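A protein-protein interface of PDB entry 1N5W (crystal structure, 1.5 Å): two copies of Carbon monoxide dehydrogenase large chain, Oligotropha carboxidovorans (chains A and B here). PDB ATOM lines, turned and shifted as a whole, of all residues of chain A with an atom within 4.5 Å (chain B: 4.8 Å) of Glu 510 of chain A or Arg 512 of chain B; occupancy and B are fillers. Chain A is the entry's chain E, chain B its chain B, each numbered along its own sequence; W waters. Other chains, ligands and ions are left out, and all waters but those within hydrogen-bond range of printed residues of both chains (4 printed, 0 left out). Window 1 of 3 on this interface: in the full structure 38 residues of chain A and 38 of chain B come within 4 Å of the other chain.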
ATOM      1  N   ALA A 509     -18.093  -3.449  -5.161  1.00  0.00           N
ATOM      2  CA  ALA A 509     -17.943  -4.622  -5.977  1.00  0.00           C
ATOM      3  C   ALA A 509     -16.533  -4.737  -6.504  1.00  0.00           C
ATOM      4  O   ALA A 509     -15.898  -3.735  -6.907  1.00  0.00           O
ATOM      5  CB  ALA A 509     -18.923  -4.585  -7.145  1.00  0.00           C
ATOM      6  N   GLU A 510     -16.007  -5.954  -6.529  1.00  0.00           N
ATOM      7  CA  GLU A 510     -14.720  -6.304  -7.178  1.00  0.00           C
ATOM      8  C   GLU A 510     -14.949  -7.461  -8.122  1.00  0.00           C
ATOM      9  O   GLU A 510     -15.512  -8.460  -7.749  1.00  0.00           O
ATOM     10  CB  GLU A 510     -13.624  -6.641  -6.170  1.00  0.00           C
ATOM     11  CG  GLU A 510     -12.290  -7.045  -6.842  1.00  0.00           C
ATOM     12  CD  GLU A 510     -11.099  -6.938  -5.931  1.00  0.00           C
ATOM     13  OE1 GLU A 510     -11.199  -7.203  -4.704  1.00  0.00           O
ATOM     14  OE2 GLU A 510     -10.014  -6.570  -6.441  1.00  0.00           O
ATOM     15  N   ILE A 511     -14.528  -7.278  -9.382  1.00  0.00           N
ATOM     16  CA  ILE A 511     -14.766  -8.270 -10.447  1.00  0.00           C
ATOM     17  C   ILE A 511     -13.425  -8.577 -11.069  1.00  0.00           C
ATOM     18  O   ILE A 511     -12.735  -7.672 -11.546  1.00  0.00           O
ATOM     19  CB  ILE A 511     -15.741  -7.668 -11.465  1.00  0.00           C
ATOM     20  CG1 ILE A 511     -17.071  -7.189 -10.888  1.00  0.00           C
ATOM     21  CG2 ILE A 511     -15.936  -8.666 -12.660  1.00  0.00           C
ATOM     22  CD1 ILE A 511     -17.983  -6.493 -11.883  1.00  0.00           C
ATOM     23  N   ARG A 512     -13.091  -9.866 -11.211  1.00  0.00           N
ATOM     24  CA  ARG A 512     -11.831 -10.326 -11.786  1.00  0.00           C
ATOM     25  C   ARG A 512     -12.096 -11.397 -12.833  1.00  0.00           C
ATOM     26  O   ARG A 512     -12.771 -12.398 -12.510  1.00  0.00           O
ATOM     27  CB  ARG A 512     -10.966 -10.931 -10.693  1.00  0.00           C
ATOM     28  CG  ARG A 512      -9.653 -11.556 -11.169  1.00  0.00           C
ATOM     29  CD  ARG A 512      -8.723 -11.975 -10.007  1.00  0.00           C
ATOM     30  NE  ARG A 512      -8.159 -10.796  -9.374  1.00  0.00           N
ATOM     31  CZ  ARG A 512      -8.212 -10.512  -8.073  1.00  0.00           C
ATOM     32  NH1 ARG A 512      -8.589 -11.449  -7.193  1.00  0.00           N
ATOM     33  NH2 ARG A 512      -7.807  -9.298  -7.676  1.00  0.00           N
ATOM     34  N   ILE A 520     -14.600 -14.281 -11.050  1.00  0.00           N
ATOM     35  CA  ILE A 520     -14.906 -14.231  -9.615  1.00  0.00           C
ATOM     36  C   ILE A 520     -15.246 -12.793  -9.231  1.00  0.00           C
ATOM     37  O   ILE A 520     -14.484 -11.858  -9.576  1.00  0.00           O
ATOM     38  CB  ILE A 520     -13.778 -14.804  -8.695  1.00  0.00           C
ATOM     39  CG1 ILE A 520     -14.068 -14.625  -7.230  1.00  0.00           C
ATOM     40  CG2 ILE A 520     -12.418 -14.192  -8.982  1.00  0.00           C
ATOM     41  CD1 ILE A 520     -15.264 -15.409  -6.708  1.00  0.00           C
ATOM     42  N   ALA A 521     -16.409 -12.588  -8.613  1.00  0.00           N
ATOM     43  CA  ALA A 521     -16.850 -11.255  -8.195  1.00  0.00           C
ATOM     44  C   ALA A 521     -17.347 -11.297  -6.754  1.00  0.00           C
ATOM     45  O   ALA A 521     -18.010 -12.273  -6.334  1.00  0.00           O
ATOM     46  CB  ALA A 521     -17.955 -10.721  -9.121  1.00  0.00           C
ATOM     47  N   ARG A 522     -17.017 -10.263  -5.999  1.00  0.00           N
ATOM     48  CA  ARG A 522     -17.449 -10.156  -4.609  1.00  0.00           C
ATOM     49  C   ARG A 522     -18.018  -8.777  -4.321  1.00  0.00           C
ATOM     50  O   ARG A 522     -17.602  -7.800  -4.976  1.00  0.00           O
ATOM     51  CB  ARG A 522     -16.255 -10.395  -3.681  1.00  0.00           C
ATOM     52  CG  ARG A 522     -15.585 -11.779  -3.885  1.00  0.00           C
ATOM     53  CD  ARG A 522     -14.668 -12.124  -2.734  1.00  0.00           C
ATOM     54  NE  ARG A 522     -14.131 -13.482  -2.859  1.00  0.00           N
ATOM     55  CZ  ARG A 522     -13.080 -13.805  -3.558  1.00  0.00           C
ATOM     56  NH1 ARG A 522     -12.310 -12.861  -4.076  1.00  0.00           N
ATOM     57  NH2 ARG A 522     -12.721 -15.080  -3.719  1.00  0.00           N
ATOM     58  N   THR A 560     -11.942 -11.236   2.268  1.00  0.00           N
ATOM     59  CA  THR A 560     -11.902 -11.337   0.813  1.00  0.00           C
ATOM     60  C   THR A 560     -12.843 -10.383   0.062  1.00  0.00           C
ATOM     61  O   THR A 560     -12.468  -9.821  -0.965  1.00  0.00           O
ATOM     62  CB  THR A 560     -12.202 -12.788   0.378  1.00  0.00           C
ATOM     63  OG1 THR A 560     -13.551 -13.130   0.667  1.00  0.00           O
ATOM     64  CG2 THR A 560     -11.287 -13.863   1.076  1.00  0.00           C
ATOM     65  N   ALA A 561     -14.024 -10.169   0.598  1.00  0.00           N
ATOM     66  CA  ALA A 561     -14.968  -9.229  -0.001  1.00  0.00           C
ATOM     67  C   ALA A 561     -14.506  -7.802   0.179  1.00  0.00           C
ATOM     68  O   ALA A 561     -13.994  -7.462   1.237  1.00  0.00           O
ATOM     69  CB  ALA A 561     -16.374  -9.404   0.573  1.00  0.00           C
ATOM     70  N   PRO A 562     -14.747  -6.926  -0.796  1.00  0.00           N
ATOM     71  CA  PRO A 562     -14.403  -5.508  -0.598  1.00  0.00           C
ATOM     72  C   PRO A 562     -15.239  -4.930   0.538  1.00  0.00           C
ATOM     73  O   PRO A 562     -16.305  -5.470   0.839  1.00  0.00           O
ATOM     74  CB  PRO A 562     -14.733  -4.859  -1.928  1.00  0.00           C
ATOM     75  CG  PRO A 562     -15.887  -5.730  -2.481  1.00  0.00           C
ATOM     76  CD  PRO A 562     -15.530  -7.149  -2.015  1.00  0.00           C
ATOM     77  N   GLU A 645      -9.607  -6.698 -14.649  1.00  0.00           N
ATOM     78  CA  GLU A 645     -10.339  -6.675 -13.411  1.00  0.00           C
ATOM     79  C   GLU A 645     -10.626  -5.240 -13.000  1.00  0.00           C
ATOM     80  O   GLU A 645      -9.960  -4.300 -13.488  1.00  0.00           O
ATOM     81  CB  GLU A 645      -9.600  -7.441 -12.339  1.00  0.00           C
ATOM     82  CG  GLU A 645      -8.205  -6.920 -11.998  1.00  0.00           C
ATOM     83  CD  GLU A 645      -7.534  -7.742 -10.929  1.00  0.00           C
ATOM     84  OE1 GLU A 645      -7.466  -7.339  -9.748  1.00  0.00           O
ATOM     85  OE2 GLU A 645      -7.137  -8.905 -11.240  1.00  0.00           O
ATOM     86  N   ALA A 646     -11.548  -5.047 -12.047  1.00  0.00           N
ATOM     87  CA  ALA A 646     -11.823  -3.729 -11.512  1.00  0.00           C
ATOM     88  C   ALA A 646     -12.554  -3.784 -10.189  1.00  0.00           C
ATOM     89  O   ALA A 646     -13.220  -4.794  -9.868  1.00  0.00           O
ATOM     90  CB  ALA A 646     -12.637  -2.866 -12.505  1.00  0.00           C
ATOM     91  N   VAL A 647     -12.496  -2.650  -9.521  1.00  0.00           N
ATOM     92  CA  VAL A 647     -13.198  -2.395  -8.281  1.00  0.00           C
ATOM     93  C   VAL A 647     -14.002  -1.078  -8.432  1.00  0.00           C
ATOM     94  O   VAL A 647     -13.522  -0.123  -9.065  1.00  0.00           O
ATOM     95  CB  VAL A 647     -12.204  -2.268  -7.107  1.00  0.00           C
ATOM     96  CG1 VAL A 647     -12.819  -1.787  -5.802  1.00  0.00           C
ATOM     97  CG2 VAL A 647     -11.450  -3.526  -6.864  1.00  0.00           C
ATOM     98  N   TYR A 649     -16.186   1.430  -5.480  1.00  0.00           N
ATOM     99  CA  TYR A 649     -16.851   1.774  -4.234  1.00  0.00           C
ATOM    100  C   TYR A 649     -17.817   2.904  -4.602  1.00  0.00           C
ATOM    101  O   TYR A 649     -17.366   3.979  -4.991  1.00  0.00           O
ATOM    102  CB  TYR A 649     -15.851   2.200  -3.142  1.00  0.00           C
ATOM    103  CG  TYR A 649     -15.126   1.065  -2.436  1.00  0.00           C
ATOM    104  CD1 TYR A 649     -14.437   0.088  -3.130  1.00  0.00           C
ATOM    105  CD2 TYR A 649     -15.117   0.959  -1.056  1.00  0.00           C
ATOM    106  CE1 TYR A 649     -13.752  -0.912  -2.463  1.00  0.00           C
ATOM    107  CE2 TYR A 649     -14.426   0.014  -0.394  1.00  0.00           C
ATOM    108  CZ  TYR A 649     -13.754  -0.978  -1.101  1.00  0.00           C
ATOM    109  OH  TYR A 649     -13.097  -1.955  -0.384  1.00  0.00           O
ATOM    110  N   GLU B 510      -2.138  -6.895  -4.762  1.00  0.00           N
ATOM    111  CA  GLU B 510      -3.378  -6.173  -4.405  1.00  0.00           C
ATOM    112  C   GLU B 510      -3.242  -5.784  -2.938  1.00  0.00           C
ATOM    113  O   GLU B 510      -2.925  -6.637  -2.109  1.00  0.00           O
ATOM    114  CB  GLU B 510      -4.650  -7.039  -4.607  1.00  0.00           C
ATOM    115  CG  GLU B 510      -5.909  -6.311  -4.188  1.00  0.00           C
ATOM    116  CD  GLU B 510      -7.195  -6.798  -4.801  1.00  0.00           C
ATOM    117  OE1 GLU B 510      -7.337  -8.033  -5.011  1.00  0.00           O
ATOM    118  OE2 GLU B 510      -8.123  -5.950  -5.065  1.00  0.00           O
ATOM    119  N   ILE B 511      -3.478  -4.507  -2.620  1.00  0.00           N
ATOM    120  CA  ILE B 511      -3.279  -3.996  -1.251  1.00  0.00           C
ATOM    121  C   ILE B 511      -4.569  -3.270  -0.852  1.00  0.00           C
ATOM    122  O   ILE B 511      -4.984  -2.340  -1.574  1.00  0.00           O
ATOM    123  CB  ILE B 511      -2.102  -3.004  -1.239  1.00  0.00           C
ATOM    124  CG1 ILE B 511      -0.805  -3.633  -1.771  1.00  0.00           C
ATOM    125  CG2 ILE B 511      -1.934  -2.423   0.156  1.00  0.00           C
ATOM    126  CD1 ILE B 511       0.342  -2.638  -1.888  1.00  0.00           C
ATOM    127  N   ARG B 512      -5.145  -3.626   0.288  1.00  0.00           N
ATOM    128  CA  ARG B 512      -6.384  -3.009   0.780  1.00  0.00           C
ATOM    129  C   ARG B 512      -6.185  -2.479   2.177  1.00  0.00           C
ATOM    130  O   ARG B 512      -5.794  -3.241   3.056  1.00  0.00           O
ATOM    131  CB  ARG B 512      -7.548  -4.004   0.669  1.00  0.00           C
ATOM    132  CG  ARG B 512      -8.863  -3.540   1.304  1.00  0.00           C
ATOM    133  CD  ARG B 512      -9.949  -4.543   1.089  1.00  0.00           C
ATOM    134  NE  ARG B 512     -10.335  -4.517  -0.324  1.00  0.00           N
ATOM    135  CZ  ARG B 512     -10.410  -5.609  -1.094  1.00  0.00           C
ATOM    136  NH1 ARG B 512     -10.306  -6.813  -0.552  1.00  0.00           N
ATOM    137  NH2 ARG B 512     -10.547  -5.469  -2.395  1.00  0.00           N
ATOM    138  N   ILE B 513      -6.405  -1.162   2.414  1.00  0.00           N
ATOM    139  CA  ILE B 513      -6.259  -0.579   3.738  1.00  0.00           C
ATOM    140  C   ILE B 513      -7.652  -0.516   4.409  1.00  0.00           C
ATOM    141  O   ILE B 513      -8.639  -0.038   3.822  1.00  0.00           O
ATOM    142  CB  ILE B 513      -5.669   0.823   3.682  1.00  0.00           C
ATOM    143  CG1 ILE B 513      -4.435   0.939   2.741  1.00  0.00           C
ATOM    144  CG2 ILE B 513      -5.404   1.304   5.090  1.00  0.00           C
ATOM    145  CD1 ILE B 513      -3.730   2.182   2.917  1.00  0.00           C
ATOM    146  N   HIS B 514      -7.741  -1.036   5.650  1.00  0.00           N
ATOM    147  CA  HIS B 514      -8.953  -1.058   6.432  1.00  0.00           C
ATOM    148  C   HIS B 514      -9.237   0.300   7.097  1.00  0.00           C
ATOM    149  O   HIS B 514      -8.348   1.147   7.170  1.00  0.00           O
ATOM    150  CB  HIS B 514      -8.843  -2.145   7.492  1.00  0.00           C
ATOM    151  CG  HIS B 514      -8.660  -3.505   6.904  1.00  0.00           C
ATOM    152  ND1 HIS B 514      -9.385  -3.922   5.799  1.00  0.00           N
ATOM    153  CD2 HIS B 514      -7.941  -4.577   7.335  1.00  0.00           C
ATOM    154  CE1 HIS B 514      -9.055  -5.173   5.548  1.00  0.00           C
ATOM    155  NE2 HIS B 514      -8.217  -5.605   6.482  1.00  0.00           N
ATOM    156  N   SER B 518      -4.959  -0.875   9.387  1.00  0.00           N
ATOM    157  CA  SER B 518      -4.282  -2.117   9.073  1.00  0.00           C
ATOM    158  C   SER B 518      -4.619  -2.551   7.661  1.00  0.00           C
ATOM    159  O   SER B 518      -5.389  -1.867   6.978  1.00  0.00           O
ATOM    160  CB  SER B 518      -4.657  -3.171  10.110  1.00  0.00           C
ATOM    161  OG  SER B 518      -6.045  -3.378  10.121  1.00  0.00           O
ATOM    162  N   VAL B 519      -3.922  -3.586   7.179  1.00  0.00           N
ATOM    163  CA  VAL B 519      -3.852  -3.878   5.748  1.00  0.00           C
ATOM    164  C   VAL B 519      -3.915  -5.382   5.470  1.00  0.00           C
ATOM    165  O   VAL B 519      -3.265  -6.148   6.179  1.00  0.00           O
ATOM    166  CB  VAL B 519      -2.486  -3.341   5.173  1.00  0.00           C
ATOM    167  CG1 VAL B 519      -2.403  -3.628   3.687  1.00  0.00           C
ATOM    168  CG2 VAL B 519      -2.283  -1.872   5.513  1.00  0.00           C
ATOM    169  N   ILE B 520      -4.636  -5.756   4.412  1.00  0.00           N
ATOM    170  CA  ILE B 520      -4.560  -7.087   3.814  1.00  0.00           C
ATOM    171  C   ILE B 520      -3.965  -6.914   2.415  1.00  0.00           C
ATOM    172  O   ILE B 520      -4.428  -6.092   1.603  1.00  0.00           O
ATOM    173  CB  ILE B 520      -5.883  -7.862   3.784  1.00  0.00           C
ATOM    174  CG1 ILE B 520      -5.733  -9.200   3.078  1.00  0.00           C
ATOM    175  CG2 ILE B 520      -7.029  -7.109   3.163  1.00  0.00           C
ATOM    176  CD1 ILE B 520      -4.887 -10.242   3.718  1.00  0.00           C
ATOM    177  N   TYR B 633     -12.899   6.446   4.283  1.00  0.00           N
ATOM    178  CA  TYR B 633     -14.170   5.746   4.575  1.00  0.00           C
ATOM    179  C   TYR B 633     -15.208   6.697   5.241  1.00  0.00           C
ATOM    180  O   TYR B 633     -16.403   6.574   4.997  1.00  0.00           O
ATOM    181  CB  TYR B 633     -13.937   4.569   5.520  1.00  0.00           C
ATOM    182  CG  TYR B 633     -13.216   3.374   4.933  1.00  0.00           C
ATOM    183  CD1 TYR B 633     -11.842   3.283   4.995  1.00  0.00           C
ATOM    184  CD2 TYR B 633     -13.897   2.300   4.380  1.00  0.00           C
ATOM    185  CE1 TYR B 633     -11.164   2.198   4.461  1.00  0.00           C
ATOM    186  CE2 TYR B 633     -13.258   1.193   3.861  1.00  0.00           C
ATOM    187  CZ  TYR B 633     -11.857   1.150   3.922  1.00  0.00           C
ATOM    188  OH  TYR B 633     -11.225   0.020   3.439  1.00  0.00           O
ATOM    189  N   LEU B 644      -9.602   2.841   0.231  1.00  0.00           N
ATOM    190  CA  LEU B 644      -8.184   3.081  -0.003  1.00  0.00           C
ATOM    191  C   LEU B 644      -7.470   1.773  -0.306  1.00  0.00           C
ATOM    192  O   LEU B 644      -7.073   1.045   0.608  1.00  0.00           O
ATOM    193  CB  LEU B 644      -7.544   3.811   1.182  1.00  0.00           C
ATOM    194  CG  LEU B 644      -6.163   4.407   0.961  1.00  0.00           C
ATOM    195  CD1 LEU B 644      -6.099   5.391  -0.202  1.00  0.00           C
ATOM    196  CD2 LEU B 644      -5.605   5.072   2.216  1.00  0.00           C
ATOM    197  N   GLU B 645      -7.364   1.439  -1.589  1.00  0.00           N
ATOM    198  CA  GLU B 645      -6.822   0.190  -2.044  1.00  0.00           C
ATOM    199  C   GLU B 645      -6.285   0.357  -3.476  1.00  0.00           C
ATOM    200  O   GLU B 645      -6.648   1.288  -4.213  1.00  0.00           O
ATOM    201  CB  GLU B 645      -7.854  -0.921  -1.868  1.00  0.00           C
ATOM    202  CG  GLU B 645      -9.109  -0.724  -2.707  1.00  0.00           C
ATOM    203  CD  GLU B 645     -10.129  -1.851  -2.427  1.00  0.00           C
ATOM    204  OE1 GLU B 645     -10.687  -1.918  -1.306  1.00  0.00           O
ATOM    205  OE2 GLU B 645     -10.221  -2.748  -3.323  1.00  0.00           O
ATOM    206  N   VAL B 647      -4.376  -2.207  -7.002  1.00  0.00           N
ATOM    207  CA  VAL B 647      -3.819  -3.388  -7.656  1.00  0.00           C
ATOM    208  C   VAL B 647      -2.782  -2.922  -8.665  1.00  0.00           C
ATOM    209  O   VAL B 647      -2.976  -1.864  -9.278  1.00  0.00           O
ATOM    210  CB  VAL B 647      -4.967  -4.136  -8.408  1.00  0.00           C
ATOM    211  CG1 VAL B 647      -4.443  -5.259  -9.292  1.00  0.00           C
ATOM    212  CG2 VAL B 647      -5.989  -4.696  -7.416  1.00  0.00           C
HETATM  213  O   HOH W   1     -11.474  -7.370   2.177  1.00  0.00           O
HETATM  214  O   HOH W   2      -9.841  -9.285  -2.124  1.00  0.00           O
HETATM  215  O   HOH W   3     -10.715   0.191   0.552  1.00  0.00           O
HETATM  216  O   HOH W   4      -9.374 -10.409  -4.454  1.00  0.00           O
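Water W1 lies within hydrogen-bond range of the backbone carbonyl oxygen (O) of Ala 561 of chain A and the guanidinium group (NH1) of Arg 512 of chain B. Water W3 lies within hydrogen-bond range of OE1 of Glu 645 of chain B (2.8 Å), N of Leu 644 of chain B (2.9 Å), OH of Tyr 633 of chain B (2.9 Å) and OH of Tyr 649 of chain A (3.3 Å). Water W2 bridges O of Thr 560 of chain A (2.9 Å) and NH1 of Arg 512 of chain B (3.0 Å). Water W4 lies within hydrogen-bond range of the guanidinium group (NH1) of Arg 512 of chain A and the side-chain carboxylate (OE1) of Glu 510 of chain B.
Glu 510 of chain A touches its own counterpart, Glu 510 of chain B. Glu 510 of chain A touches Arg 512 of chain B, and with the chains exchanged Arg 512 of chain A touches Glu 510 of chain B. Glu 645 of chain A touches Val 647 of chain B, and with the chains exchanged Val 647 of chain A touches Glu 645 of chain B. Positions printed for both chains: 510, 511, 512, 520, 645 and 647.
OE2 of Glu 510 of chain A sits close to OE2 of Glu 510 of chain B (2.4 Å). OE1 of Glu 510 of chain B is in salt-bridge range of NH2 of Arg 512 of chain A. The guanidinium group of Arg 512 of chain B lies within salt-bridge range of the side-chain carboxylate of Glu 510 of chain A (3.0 Å). OH of Tyr 649 of chain A lies within hydrogen-bond range of OE1 of Glu 645 of chain B (2.6 Å).
OE2 of Glu 510 of chain B lies within salt-bridge range of NH2 of Arg 512 of chain B, 3.6 Å away. N of Arg 512 of chain B sits at hydrogen-bond distance from O of Ile 520 of chain B. OE1 of Glu 645 of chain B lies within salt-bridge range of NE of Arg 512 of chain B, 2.8 Å away. The guanidinium group (NH2) of Arg 512 of chain A lies within salt-bridge range of the side-chain carboxylate (OE2) of Glu 510 of chain A. The backbone NH of Arg 512 of chain A sits at hydrogen-bond distance from the backbone carbonyl oxygen of Ile 520 of chain A (2.9 Å). The side-chain carboxylate (OE2) of Glu 645 of chain A is in salt-bridge range of the guanidinium group (NE) of Arg 512 of chain A (2.8 Å).
Of the 14 printed residues of chain A, 6 touch a printed residue of chain B. Hydrophobic or aromatic side chains of chain A that line the printed part of chain B: Val 647 and Tyr 649. Along chain A the printed residues that touch a printed residue of chain B span positions 510 to 649. Hydrophobic or aromatic side chains of chain B within 4 Å of the printed part of chain A: Val 647. Among the printed residues, Asp or Glu carboxylates within 4 Å of a Lys or Arg side-chain nitrogen of the other chain: Glu 510 of chain A with Arg 512 of chain B (3.0 Å) and Arg 512 of chain A with Glu 510 of chain B (3.0 Å).
Thr 560 of chain A touches Arg 512 of chain B. CG1 of Val 647 of chain B touches OE1 of Glu 645 of chain A, at 3.7 Å. Val 647 of chain A touches Glu 645 of chain B (CG1 to OE2, 3.7 Å). Arg 512 of chain B touches Tyr 649 of chain A (NE to OH, 3.8 Å).
Glu 510 of chain A touches just these residues of chain B: Glu 510 (2.4 Å) and Arg 512 (3.0 Å). Arg 512 of chain B touches just these residues of chain A: Glu 510 (3.0 Å), Thr 560 (3.7 Å) and Tyr 649 (3.8 Å). Of the printed residues of chain A, Val 647 of chain B touches Glu 645 (3.7 Å). Printed residues of chain B within 4 Å of Thr 560 of chain A: Arg 512. Printed residues of chain B within 4 Å of Arg 512 of chain A: Glu 510 (3.0 Å). Printed residues of chain B within 4 Å of Val 647 of chain A: Glu 645. Of the printed residues of chain A, Glu 510 of chain B touches Glu 510 (2.4 Å) and Arg 512 (3.0 Å). The nearest residue of chain A that does not touch Arg 512 of chain B is Pro 562 of chain A (4.02 Å). The nearest printed residue of chain A that does not touch Val 647 of chain B is Glu 510 of chain A (4.5 Å).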
